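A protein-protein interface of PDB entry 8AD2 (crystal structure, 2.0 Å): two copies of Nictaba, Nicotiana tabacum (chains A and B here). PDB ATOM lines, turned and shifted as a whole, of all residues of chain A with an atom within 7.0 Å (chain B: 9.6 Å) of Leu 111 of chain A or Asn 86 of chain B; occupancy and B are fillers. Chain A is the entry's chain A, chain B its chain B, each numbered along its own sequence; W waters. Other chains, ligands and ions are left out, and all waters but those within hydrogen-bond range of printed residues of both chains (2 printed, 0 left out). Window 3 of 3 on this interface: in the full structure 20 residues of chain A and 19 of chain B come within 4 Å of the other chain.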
ATOM      1  N   PHE A 100     -14.788   3.248 -22.151  1.00  0.00           N
ATOM      2  CA  PHE A 100     -14.893   3.116 -23.607  1.00  0.00           C
ATOM      3  C   PHE A 100     -15.339   4.441 -24.218  1.00  0.00           C
ATOM      4  O   PHE A 100     -16.175   5.157 -23.650  1.00  0.00           O
ATOM      5  CB  PHE A 100     -15.881   2.016 -23.985  1.00  0.00           C
ATOM      6  CG  PHE A 100     -15.412   0.612 -23.628  1.00  0.00           C
ATOM      7  CD1 PHE A 100     -14.328   0.052 -24.257  1.00  0.00           C
ATOM      8  CD2 PHE A 100     -16.064  -0.127 -22.651  1.00  0.00           C
ATOM      9  CE1 PHE A 100     -13.892  -1.229 -23.923  1.00  0.00           C
ATOM     10  CE2 PHE A 100     -15.634  -1.419 -22.328  1.00  0.00           C
ATOM     11  CZ  PHE A 100     -14.557  -1.956 -22.963  1.00  0.00           C
ATOM     12  N   LYS A 103     -15.622   2.589 -28.939  1.00  0.00           N
ATOM     13  CA  LYS A 103     -16.160   1.246 -29.089  1.00  0.00           C
ATOM     14  C   LYS A 103     -17.647   1.236 -28.773  1.00  0.00           C
ATOM     15  O   LYS A 103     -18.095   1.874 -27.811  1.00  0.00           O
ATOM     16  CB  LYS A 103     -15.419   0.275 -28.175  1.00  0.00           C
ATOM     17  CG  LYS A 103     -15.635  -1.201 -28.528  1.00  0.00           C
ATOM     18  CD  LYS A 103     -15.008  -2.109 -27.482  1.00  0.00           C
ATOM     19  CE  LYS A 103     -15.884  -3.333 -27.167  1.00  0.00           C
ATOM     20  NZ  LYS A 103     -16.788  -3.764 -28.274  1.00  0.00           N
ATOM     21  N   LYS A 105     -21.103  -0.764 -27.644  1.00  0.00           N
ATOM     22  CA  LYS A 105     -21.499  -1.907 -26.842  1.00  0.00           C
ATOM     23  C   LYS A 105     -22.005  -3.011 -27.765  1.00  0.00           C
ATOM     24  O   LYS A 105     -22.985  -2.825 -28.495  1.00  0.00           O
ATOM     25  CB  LYS A 105     -22.576  -1.519 -25.822  1.00  0.00           C
ATOM     26  CG  LYS A 105     -22.815  -2.585 -24.720  1.00  0.00           C
ATOM     27  CD  LYS A 105     -23.329  -1.989 -23.421  1.00  0.00           C
ATOM     28  CE  LYS A 105     -23.093  -2.924 -22.214  1.00  0.00           C
ATOM     29  NZ  LYS A 105     -22.601  -2.229 -20.938  1.00  0.00           N
ATOM     30  N   LEU A 107     -22.859  -6.698 -27.124  1.00  0.00           N
ATOM     31  CA  LEU A 107     -23.869  -7.594 -26.604  1.00  0.00           C
ATOM     32  C   LEU A 107     -24.294  -7.095 -25.238  1.00  0.00           C
ATOM     33  O   LEU A 107     -23.470  -6.544 -24.492  1.00  0.00           O
ATOM     34  CB  LEU A 107     -23.321  -9.024 -26.512  1.00  0.00           C
ATOM     35  CG  LEU A 107     -22.626  -9.462 -27.814  1.00  0.00           C
ATOM     36  CD1 LEU A 107     -21.411 -10.320 -27.578  1.00  0.00           C
ATOM     37  CD2 LEU A 107     -23.637 -10.195 -28.726  1.00  0.00           C
ATOM     38  N   PRO A 108     -25.568  -7.230 -24.890  1.00  0.00           N
ATOM     39  CA  PRO A 108     -26.057  -6.557 -23.672  1.00  0.00           C
ATOM     40  C   PRO A 108     -25.277  -6.913 -22.411  1.00  0.00           C
ATOM     41  O   PRO A 108     -25.282  -6.120 -21.459  1.00  0.00           O
ATOM     42  CB  PRO A 108     -27.526  -6.999 -23.578  1.00  0.00           C
ATOM     43  CG  PRO A 108     -27.897  -7.380 -24.991  1.00  0.00           C
ATOM     44  CD  PRO A 108     -26.632  -7.972 -25.597  1.00  0.00           C
ATOM     45  N   GLY A 109     -24.586  -8.056 -22.381  1.00  0.00           N
ATOM     46  CA  GLY A 109     -23.801  -8.458 -21.227  1.00  0.00           C
ATOM     47  C   GLY A 109     -22.407  -7.878 -21.127  1.00  0.00           C
ATOM     48  O   GLY A 109     -21.668  -8.192 -20.187  1.00  0.00           O
ATOM     49  N   GLU A 110     -22.025  -7.033 -22.074  1.00  0.00           N
ATOM     50  CA  GLU A 110     -20.682  -6.482 -22.087  1.00  0.00           C
ATOM     51  C   GLU A 110     -20.532  -5.457 -20.975  1.00  0.00           C
ATOM     52  O   GLU A 110     -21.374  -4.574 -20.815  1.00  0.00           O
ATOM     53  CB  GLU A 110     -20.391  -5.841 -23.443  1.00  0.00           C
ATOM     54  CG  GLU A 110     -18.904  -5.825 -23.797  1.00  0.00           C
ATOM     55  CD  GLU A 110     -18.642  -5.200 -25.146  1.00  0.00           C
ATOM     56  OE1 GLU A 110     -17.464  -5.052 -25.515  1.00  0.00           O
ATOM     57  OE2 GLU A 110     -19.615  -4.858 -25.841  1.00  0.00           O
ATOM     58  N   LEU A 111     -19.460  -5.572 -20.213  1.00  0.00           N
ATOM     59  CA  LEU A 111     -19.227  -4.696 -19.081  1.00  0.00           C
ATOM     60  C   LEU A 111     -18.463  -3.440 -19.506  1.00  0.00           C
ATOM     61  O   LEU A 111     -17.831  -3.375 -20.562  1.00  0.00           O
ATOM     62  CB  LEU A 111     -18.447  -5.425 -17.996  1.00  0.00           C
ATOM     63  CG  LEU A 111     -19.118  -6.674 -17.444  1.00  0.00           C
ATOM     64  CD1 LEU A 111     -18.422  -7.083 -16.187  1.00  0.00           C
ATOM     65  CD2 LEU A 111     -20.577  -6.444 -17.205  1.00  0.00           C
ATOM     66  N   GLY A 112     -18.498  -2.443 -18.642  1.00  0.00           N
ATOM     67  CA  GLY A 112     -17.741  -1.228 -18.841  1.00  0.00           C
ATOM     68  C   GLY A 112     -18.631   0.001 -18.901  1.00  0.00           C
ATOM     69  O   GLY A 112     -19.856  -0.068 -18.983  1.00  0.00           O
ATOM     70  N   ARG A 113     -17.973   1.137 -18.826  1.00  0.00           N
ATOM     71  CA  ARG A 113     -18.656   2.419 -18.943  1.00  0.00           C
ATOM     72  C   ARG A 113     -18.609   2.853 -20.400  1.00  0.00           C
ATOM     73  O   ARG A 113     -17.519   3.053 -20.963  1.00  0.00           O
ATOM     74  CB  ARG A 113     -18.017   3.466 -18.038  1.00  0.00           C
ATOM     75  CG  ARG A 113     -18.873   4.706 -17.880  1.00  0.00           C
ATOM     76  CD  ARG A 113     -18.211   5.721 -16.908  1.00  0.00           C
ATOM     77  NE  ARG A 113     -18.401   5.346 -15.509  1.00  0.00           N
ATOM     78  CZ  ARG A 113     -17.663   5.797 -14.503  1.00  0.00           C
ATOM     79  NH1 ARG A 113     -16.661   6.644 -14.734  1.00  0.00           N
ATOM     80  NH2 ARG A 113     -17.934   5.400 -13.264  1.00  0.00           N
ATOM     81  N   PHE A 114     -19.785   2.989 -21.001  1.00  0.00           N
ATOM     82  CA  PHE A 114     -19.897   3.386 -22.382  1.00  0.00           C
ATOM     83  C   PHE A 114     -20.513   4.776 -22.459  1.00  0.00           C
ATOM     84  O   PHE A 114     -21.184   5.230 -21.528  1.00  0.00           O
ATOM     85  CB  PHE A 114     -20.758   2.415 -23.196  1.00  0.00           C
ATOM     86  CG  PHE A 114     -20.113   1.095 -23.472  1.00  0.00           C
ATOM     87  CD1 PHE A 114     -19.481   0.856 -24.685  1.00  0.00           C
ATOM     88  CD2 PHE A 114     -20.172   0.069 -22.538  1.00  0.00           C
ATOM     89  CE1 PHE A 114     -18.906  -0.365 -24.943  1.00  0.00           C
ATOM     90  CE2 PHE A 114     -19.609  -1.160 -22.800  1.00  0.00           C
ATOM     91  CZ  PHE A 114     -18.958  -1.380 -23.992  1.00  0.00           C
ATOM     92  N   TYR B  46     -11.570  -7.761   0.611  1.00  0.00           N
ATOM     93  CA  TYR B  46     -12.485  -7.479  -0.498  1.00  0.00           C
ATOM     94  C   TYR B  46     -13.918  -7.694  -0.054  1.00  0.00           C
ATOM     95  O   TYR B  46     -14.205  -8.606   0.717  1.00  0.00           O
ATOM     96  CB  TYR B  46     -12.225  -8.404  -1.704  1.00  0.00           C
ATOM     97  CG  TYR B  46     -13.264  -8.409  -2.779  1.00  0.00           C
ATOM     98  CD1 TYR B  46     -14.415  -9.184  -2.691  1.00  0.00           C
ATOM     99  CD2 TYR B  46     -13.093  -7.622  -3.909  1.00  0.00           C
ATOM    100  CE1 TYR B  46     -15.385  -9.136  -3.713  1.00  0.00           C
ATOM    101  CE2 TYR B  46     -13.975  -7.629  -4.923  1.00  0.00           C
ATOM    102  CZ  TYR B  46     -15.130  -8.360  -4.811  1.00  0.00           C
ATOM    103  OH  TYR B  46     -15.991  -8.338  -5.830  1.00  0.00           O
ATOM    104  N   LYS B  48     -18.334  -6.816  -1.309  1.00  0.00           N
ATOM    105  CA  LYS B  48     -19.273  -6.568  -2.389  1.00  0.00           C
ATOM    106  C   LYS B  48     -20.666  -6.432  -1.794  1.00  0.00           C
ATOM    107  O   LYS B  48     -21.009  -7.167  -0.865  1.00  0.00           O
ATOM    108  CB  LYS B  48     -19.202  -7.751  -3.374  1.00  0.00           C
ATOM    109  CG  LYS B  48     -19.833  -7.523  -4.710  1.00  0.00           C
ATOM    110  CD  LYS B  48     -19.585  -8.709  -5.639  1.00  0.00           C
ATOM    111  CE  LYS B  48     -20.376  -9.915  -5.219  1.00  0.00           C
ATOM    112  NZ  LYS B  48     -20.429 -10.962  -6.261  1.00  0.00           N
ATOM    113  N   ILE B  49     -21.447  -5.478  -2.321  1.00  0.00           N
ATOM    114  CA  ILE B  49     -22.837  -5.268  -1.923  1.00  0.00           C
ATOM    115  C   ILE B  49     -23.731  -5.119  -3.153  1.00  0.00           C
ATOM    116  O   ILE B  49     -23.278  -4.779  -4.247  1.00  0.00           O
ATOM    117  CB  ILE B  49     -23.003  -4.018  -1.024  1.00  0.00           C
ATOM    118  CG1 ILE B  49     -22.723  -2.752  -1.858  1.00  0.00           C
ATOM    119  CG2 ILE B  49     -22.111  -4.087   0.207  1.00  0.00           C
ATOM    120  CD1 ILE B  49     -22.814  -1.476  -1.093  1.00  0.00           C
ATOM    121  N   GLU B  50     -25.023  -5.357  -2.962  1.00  0.00           N
ATOM    122  CA  GLU B  50     -26.045  -5.061  -3.949  1.00  0.00           C
ATOM    123  C   GLU B  50     -26.577  -3.668  -3.649  1.00  0.00           C
ATOM    124  O   GLU B  50     -26.854  -3.353  -2.489  1.00  0.00           O
ATOM    125  CB  GLU B  50     -27.168  -6.092  -3.853  1.00  0.00           C
ATOM    126  CG  GLU B  50     -26.705  -7.604  -4.098  1.00  0.00           C
ATOM    127  CD  GLU B  50     -26.604  -7.941  -5.575  1.00  0.00           C
ATOM    128  OE1 GLU B  50     -26.077  -9.047  -5.980  1.00  0.00           O
ATOM    129  OE2 GLU B  50     -27.105  -7.103  -6.391  1.00  0.00           O
ATOM    130  N   THR B  51     -26.681  -2.820  -4.663  1.00  0.00           N
ATOM    131  CA  THR B  51     -27.213  -1.477  -4.411  1.00  0.00           C
ATOM    132  C   THR B  51     -28.738  -1.463  -4.308  1.00  0.00           C
ATOM    133  O   THR B  51     -29.339  -0.453  -3.919  1.00  0.00           O
ATOM    134  CB  THR B  51     -26.768  -0.497  -5.496  1.00  0.00           C
ATOM    135  OG1 THR B  51     -27.116  -1.004  -6.787  1.00  0.00           O
ATOM    136  CG2 THR B  51     -25.287  -0.234  -5.385  1.00  0.00           C
ATOM    137  N   ARG B  83     -15.692   0.227  -7.115  1.00  0.00           N
ATOM    138  CA  ARG B  83     -16.214   0.362  -8.459  1.00  0.00           C
ATOM    139  C   ARG B  83     -17.505  -0.436  -8.570  1.00  0.00           C
ATOM    140  O   ARG B  83     -17.732  -1.399  -7.829  1.00  0.00           O
ATOM    141  CB  ARG B  83     -15.196  -0.085  -9.511  1.00  0.00           C
ATOM    142  CG  ARG B  83     -14.711  -1.510  -9.408  1.00  0.00           C
ATOM    143  CD  ARG B  83     -13.351  -1.706 -10.041  1.00  0.00           C
ATOM    144  NE  ARG B  83     -13.019  -3.129 -10.184  1.00  0.00           N
ATOM    145  CZ  ARG B  83     -12.082  -3.592 -11.008  1.00  0.00           C
ATOM    146  NH1 ARG B  83     -11.379  -2.752 -11.764  1.00  0.00           N
ATOM    147  NH2 ARG B  83     -11.845  -4.895 -11.079  1.00  0.00           N
ATOM    148  N   PHE B  84     -18.337  -0.011  -9.520  1.00  0.00           N
ATOM    149  CA  PHE B  84     -19.498  -0.786  -9.938  1.00  0.00           C
ATOM    150  C   PHE B  84     -18.985  -1.974 -10.740  1.00  0.00           C
ATOM    151  O   PHE B  84     -18.219  -1.804 -11.700  1.00  0.00           O
ATOM    152  CB  PHE B  84     -20.443   0.073 -10.780  1.00  0.00           C
ATOM    153  CG  PHE B  84     -21.343   0.937  -9.971  1.00  0.00           C
ATOM    154  CD1 PHE B  84     -22.558   0.456  -9.470  1.00  0.00           C
ATOM    155  CD2 PHE B  84     -20.971   2.237  -9.695  1.00  0.00           C
ATOM    156  CE1 PHE B  84     -23.366   1.269  -8.703  1.00  0.00           C
ATOM    157  CE2 PHE B  84     -21.811   3.094  -8.960  1.00  0.00           C
ATOM    158  CZ  PHE B  84     -23.012   2.614  -8.473  1.00  0.00           C
ATOM    159  N   VAL B  85     -19.364  -3.187 -10.324  1.00  0.00           N
ATOM    160  CA  VAL B  85     -18.914  -4.395 -11.012  1.00  0.00           C
ATOM    161  C   VAL B  85     -19.183  -4.298 -12.515  1.00  0.00           C
ATOM    162  O   VAL B  85     -18.335  -4.645 -13.337  1.00  0.00           O
ATOM    163  CB  VAL B  85     -19.595  -5.628 -10.390  1.00  0.00           C
ATOM    164  CG1 VAL B  85     -19.266  -6.871 -11.194  1.00  0.00           C
ATOM    165  CG2 VAL B  85     -19.178  -5.794  -8.925  1.00  0.00           C
ATOM    166  N   ASN B  86     -20.345  -3.800 -12.904  1.00  0.00           N
ATOM    167  CA  ASN B  86     -20.679  -3.773 -14.323  1.00  0.00           C
ATOM    168  C   ASN B  86     -19.900  -2.742 -15.140  1.00  0.00           C
ATOM    169  O   ASN B  86     -20.004  -2.751 -16.377  1.00  0.00           O
ATOM    170  CB  ASN B  86     -22.168  -3.483 -14.517  1.00  0.00           C
ATOM    171  CG  ASN B  86     -23.042  -4.470 -13.815  1.00  0.00           C
ATOM    172  OD1 ASN B  86     -22.620  -5.608 -13.558  1.00  0.00           O
ATOM    173  ND2 ASN B  86     -24.271  -4.047 -13.472  1.00  0.00           N
ATOM    174  N   GLU B  87     -19.125  -1.872 -14.496  1.00  0.00           N
ATOM    175  CA  GLU B  87     -18.430  -0.802 -15.182  1.00  0.00           C
ATOM    176  C   GLU B  87     -16.978  -1.159 -15.418  1.00  0.00           C
ATOM    177  O   GLU B  87     -16.209  -0.323 -15.875  1.00  0.00           O
ATOM    178  CB  GLU B  87     -18.560   0.510 -14.388  1.00  0.00           C
ATOM    179  CG  GLU B  87     -19.946   1.083 -14.466  1.00  0.00           C
ATOM    180  CD  GLU B  87     -20.042   2.522 -13.897  1.00  0.00           C
ATOM    181  OE1 GLU B  87     -19.032   3.089 -13.405  1.00  0.00           O
ATOM    182  OE2 GLU B  87     -21.133   3.075 -13.948  1.00  0.00           O
ATOM    183  N   VAL B  88     -16.576  -2.374 -15.100  1.00  0.00           N
ATOM    184  CA  VAL B  88     -15.187  -2.776 -15.240  1.00  0.00           C
ATOM    185  C   VAL B  88     -14.995  -3.282 -16.663  1.00  0.00           C
ATOM    186  O   VAL B  88     -15.653  -4.237 -17.084  1.00  0.00           O
ATOM    187  CB  VAL B  88     -14.826  -3.847 -14.202  1.00  0.00           C
ATOM    188  CG1 VAL B  88     -13.423  -4.370 -14.436  1.00  0.00           C
ATOM    189  CG2 VAL B  88     -14.940  -3.269 -12.808  1.00  0.00           C
ATOM    190  N   ALA B  89     -14.153  -2.599 -17.431  1.00  0.00           N
ATOM    191  CA  ALA B  89     -13.919  -2.979 -18.813  1.00  0.00           C
ATOM    192  C   ALA B  89     -13.103  -4.259 -18.881  1.00  0.00           C
ATOM    193  O   ALA B  89     -12.217  -4.472 -18.063  1.00  0.00           O
ATOM    194  CB  ALA B  89     -13.189  -1.864 -19.544  1.00  0.00           C
ATOM    195  N   GLU B  90     -13.388  -5.108 -19.859  1.00  0.00           N
ATOM    196  CA  GLU B  90     -12.674  -6.374 -19.973  1.00  0.00           C
ATOM    197  C   GLU B  90     -11.177  -6.113 -20.068  1.00  0.00           C
ATOM    198  O   GLU B  90     -10.731  -5.252 -20.835  1.00  0.00           O
ATOM    199  CB  GLU B  90     -13.164  -7.175 -21.185  1.00  0.00           C
ATOM    200  CG  GLU B  90     -12.816  -8.671 -21.056  1.00  0.00           C
ATOM    201  CD  GLU B  90     -13.630  -9.572 -21.982  1.00  0.00           C
ATOM    202  OE1 GLU B  90     -13.719  -9.260 -23.198  1.00  0.00           O
ATOM    203  OE2 GLU B  90     -14.174 -10.595 -21.495  1.00  0.00           O
ATOM    204  N   GLY B  91     -10.397  -6.818 -19.249  1.00  0.00           N
ATOM    205  CA  GLY B  91      -8.961  -6.674 -19.273  1.00  0.00           C
ATOM    206  C   GLY B  91      -8.415  -5.620 -18.353  1.00  0.00           C
ATOM    207  O   GLY B  91      -7.198  -5.576 -18.151  1.00  0.00           O
ATOM    208  N   ALA B  92      -9.271  -4.759 -17.828  1.00  0.00           N
ATOM    209  CA  ALA B  92      -8.833  -3.687 -16.927  1.00  0.00           C
ATOM    210  C   ALA B  92      -8.374  -4.344 -15.636  1.00  0.00           C
ATOM    211  O   ALA B  92      -8.987  -5.309 -15.211  1.00  0.00           O
ATOM    212  CB  ALA B  92      -9.930  -2.688 -16.687  1.00  0.00           C
ATOM    213  N   GLY B 135     -31.124   2.051  -7.379  1.00  0.00           N
ATOM    214  CA  GLY B 135     -30.807   0.663  -7.101  1.00  0.00           C
ATOM    215  C   GLY B 135     -30.771  -0.260  -8.302  1.00  0.00           C
ATOM    216  O   GLY B 135     -30.862  -1.479  -8.133  1.00  0.00           O
ATOM    217  N   GLU B 136     -30.625   0.279  -9.512  1.00  0.00           N
ATOM    218  CA  GLU B 136     -30.681  -0.508 -10.733  1.00  0.00           C
ATOM    219  C   GLU B 136     -29.326  -0.700 -11.399  1.00  0.00           C
ATOM    220  O   GLU B 136     -29.267  -1.307 -12.471  1.00  0.00           O
ATOM    221  CB  GLU B 136     -31.679   0.148 -11.722  1.00  0.00           C
ATOM    222  CG  GLU B 136     -33.174  -0.021 -11.276  1.00  0.00           C
ATOM    223  CD  GLU B 136     -34.213   0.796 -12.082  1.00  0.00           C
ATOM    224  OE1 GLU B 136     -35.424   0.525 -11.900  1.00  0.00           O
ATOM    225  OE2 GLU B 136     -33.852   1.713 -12.869  1.00  0.00           O
ATOM    226  N   ASP B 137     -28.243  -0.214 -10.805  1.00  0.00           N
ATOM    227  CA  ASP B 137     -26.935  -0.302 -11.450  1.00  0.00           C
ATOM    228  C   ASP B 137     -26.072  -1.426 -10.907  1.00  0.00           C
ATOM    229  O   ASP B 137     -24.910  -1.528 -11.297  1.00  0.00           O
ATOM    230  CB  ASP B 137     -26.169   1.025 -11.314  1.00  0.00           C
ATOM    231  CG  ASP B 137     -26.887   2.163 -11.995  1.00  0.00           C
ATOM    232  OD1 ASP B 137     -27.456   1.884 -13.057  1.00  0.00           O
ATOM    233  OD2 ASP B 137     -26.873   3.303 -11.477  1.00  0.00           O
ATOM    234  N   GLY B 138     -26.591  -2.251 -10.017  1.00  0.00           N
ATOM    235  CA  GLY B 138     -25.992  -3.538  -9.747  1.00  0.00           C
ATOM    236  C   GLY B 138     -25.128  -3.534  -8.527  1.00  0.00           C
ATOM    237  O   GLY B 138     -25.327  -2.717  -7.615  1.00  0.00           O
ATOM    238  N   GLU B 139     -24.150  -4.433  -8.524  1.00  0.00           N
ATOM    239  CA  GLU B 139     -23.259  -4.567  -7.392  1.00  0.00           C
ATOM    240  C   GLU B 139     -22.169  -3.504  -7.416  1.00  0.00           C
ATOM    241  O   GLU B 139     -21.747  -3.031  -8.463  1.00  0.00           O
ATOM    242  CB  GLU B 139     -22.621  -5.965  -7.387  1.00  0.00           C
ATOM    243  CG  GLU B 139     -23.614  -7.070  -7.437  1.00  0.00           C
ATOM    244  CD  GLU B 139     -22.930  -8.438  -7.695  1.00  0.00           C
ATOM    245  OE1 GLU B 139     -21.828  -8.459  -8.282  1.00  0.00           O
ATOM    246  OE2 GLU B 139     -23.517  -9.482  -7.318  1.00  0.00           O
ATOM    247  N   VAL B 140     -21.719  -3.139  -6.229  1.00  0.00           N
ATOM    248  CA  VAL B 140     -20.512  -2.360  -6.001  1.00  0.00           C
ATOM    249  C   VAL B 140     -19.531  -3.240  -5.249  1.00  0.00           C
ATOM    250  O   VAL B 140     -19.923  -3.930  -4.295  1.00  0.00           O
ATOM    251  CB  VAL B 140     -20.823  -1.075  -5.212  1.00  0.00           C
ATOM    252  CG1 VAL B 140     -19.537  -0.360  -4.777  1.00  0.00           C
ATOM    253  CG2 VAL B 140     -21.683  -0.137  -6.107  1.00  0.00           C
ATOM    254  N   GLU B 141     -18.273  -3.229  -5.681  1.00  0.00           N
ATOM    255  CA  GLU B 141     -17.196  -4.044  -5.083  1.00  0.00           C
ATOM    256  C   GLU B 141     -16.148  -3.083  -4.548  1.00  0.00           C
ATOM    257  O   GLU B 141     -16.071  -2.002  -5.057  1.00  0.00           O
ATOM    258  CB  GLU B 141     -16.573  -4.989  -6.109  1.00  0.00           C
ATOM    259  CG  GLU B 141     -15.797  -4.314  -7.219  1.00  0.00           C
ATOM    260  CD  GLU B 141     -15.504  -5.219  -8.397  1.00  0.00           C
ATOM    261  OE1 GLU B 141     -15.118  -6.368  -8.176  1.00  0.00           O
ATOM    262  OE2 GLU B 141     -15.692  -4.770  -9.530  1.00  0.00           O
HETATM  263  O   HOH W   1     -15.392   1.127 -17.831  1.00  0.00           O
HETATM  264  O   HOH W   2     -15.733  -4.895 -21.594  1.00  0.00           O
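N of Phe 100 of chain A is in hydrogen-bond range of O of Arg 113 of chain A (3.0 Å).
O of Glu 139 of chain B sits at hydrogen-bond distance from N of Val 85 of chain B (3.0 Å).
The backbone carbonyl oxygen of Asp 137 of chain B lies within hydrogen-bond range of the side-chain amide nitrogen of Asn 86 of chain B, 3.4 Å away.
Hydrophobic or aromatic side chains of chain B that line the printed part of chain A: Ala 89.
Along chain B the printed residues that touch a printed residue of chain A span positions 85 to 89.
CB of Ala 89 of chain B touches CZ of Phe 100 of chain A, at 3.7 Å.
Leu 111 of chain A touches Val 85 of chain B (CD1 to O, 3.8 Å).
Leu 111 of chain A touches Asn 86 of chain B (CA to O, 3.4 Å).
Leu 111 of chain A touches Val 88 of chain B.
Glu 87 of chain B touches Gly 112 of chain A.
N of Gly 112 of chain A touches O of Val 88 of chain B (3.7 Å).
Water W1 bridges the backbone carbonyl oxygen (O) of Glu 87 of chain B and the backbone NH (N) of Arg 113 of chain A.
Water W2 bridges the backbone carbonyl oxygen (O) of Leu 111 of chain A (2.8 Å) and the backbone NH (N) of Glu 90 of chain B (2.9 Å).
No position is printed for both chains.
Of the 8 pairs that touch across the chains among the printed residues, none has its exchanged pair printed and touching as well.
O of Asn 86 of chain B sits at hydrogen-bond distance from N of Gly 112 of chain A (2.7 Å).
NH2 of Arg 113 of chain A is in salt-bridge range of OE1 of Glu 87 of chain B (2.6 Å).
Leu 111 of chain A touches three residues of chain B.
Of chain B, only Asn 86 (2.7 Å), Glu 87 (3.5 Å) and Val 88 (3.7 Å) come within 4 Å of Gly 112 of chain A.
Of the printed residues of chain B, Arg 113 of chain A touches Glu 87.
Of the printed residues of chain A, Val 85 of chain B touches Leu 111.
Asn 86 of chain B touches just these residues of chain A: Leu 111 and Gly 112.
The nearest residue of chain A that does not touch Asn 86 of chain B is Glu 110 of chain A (5.0 Å).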
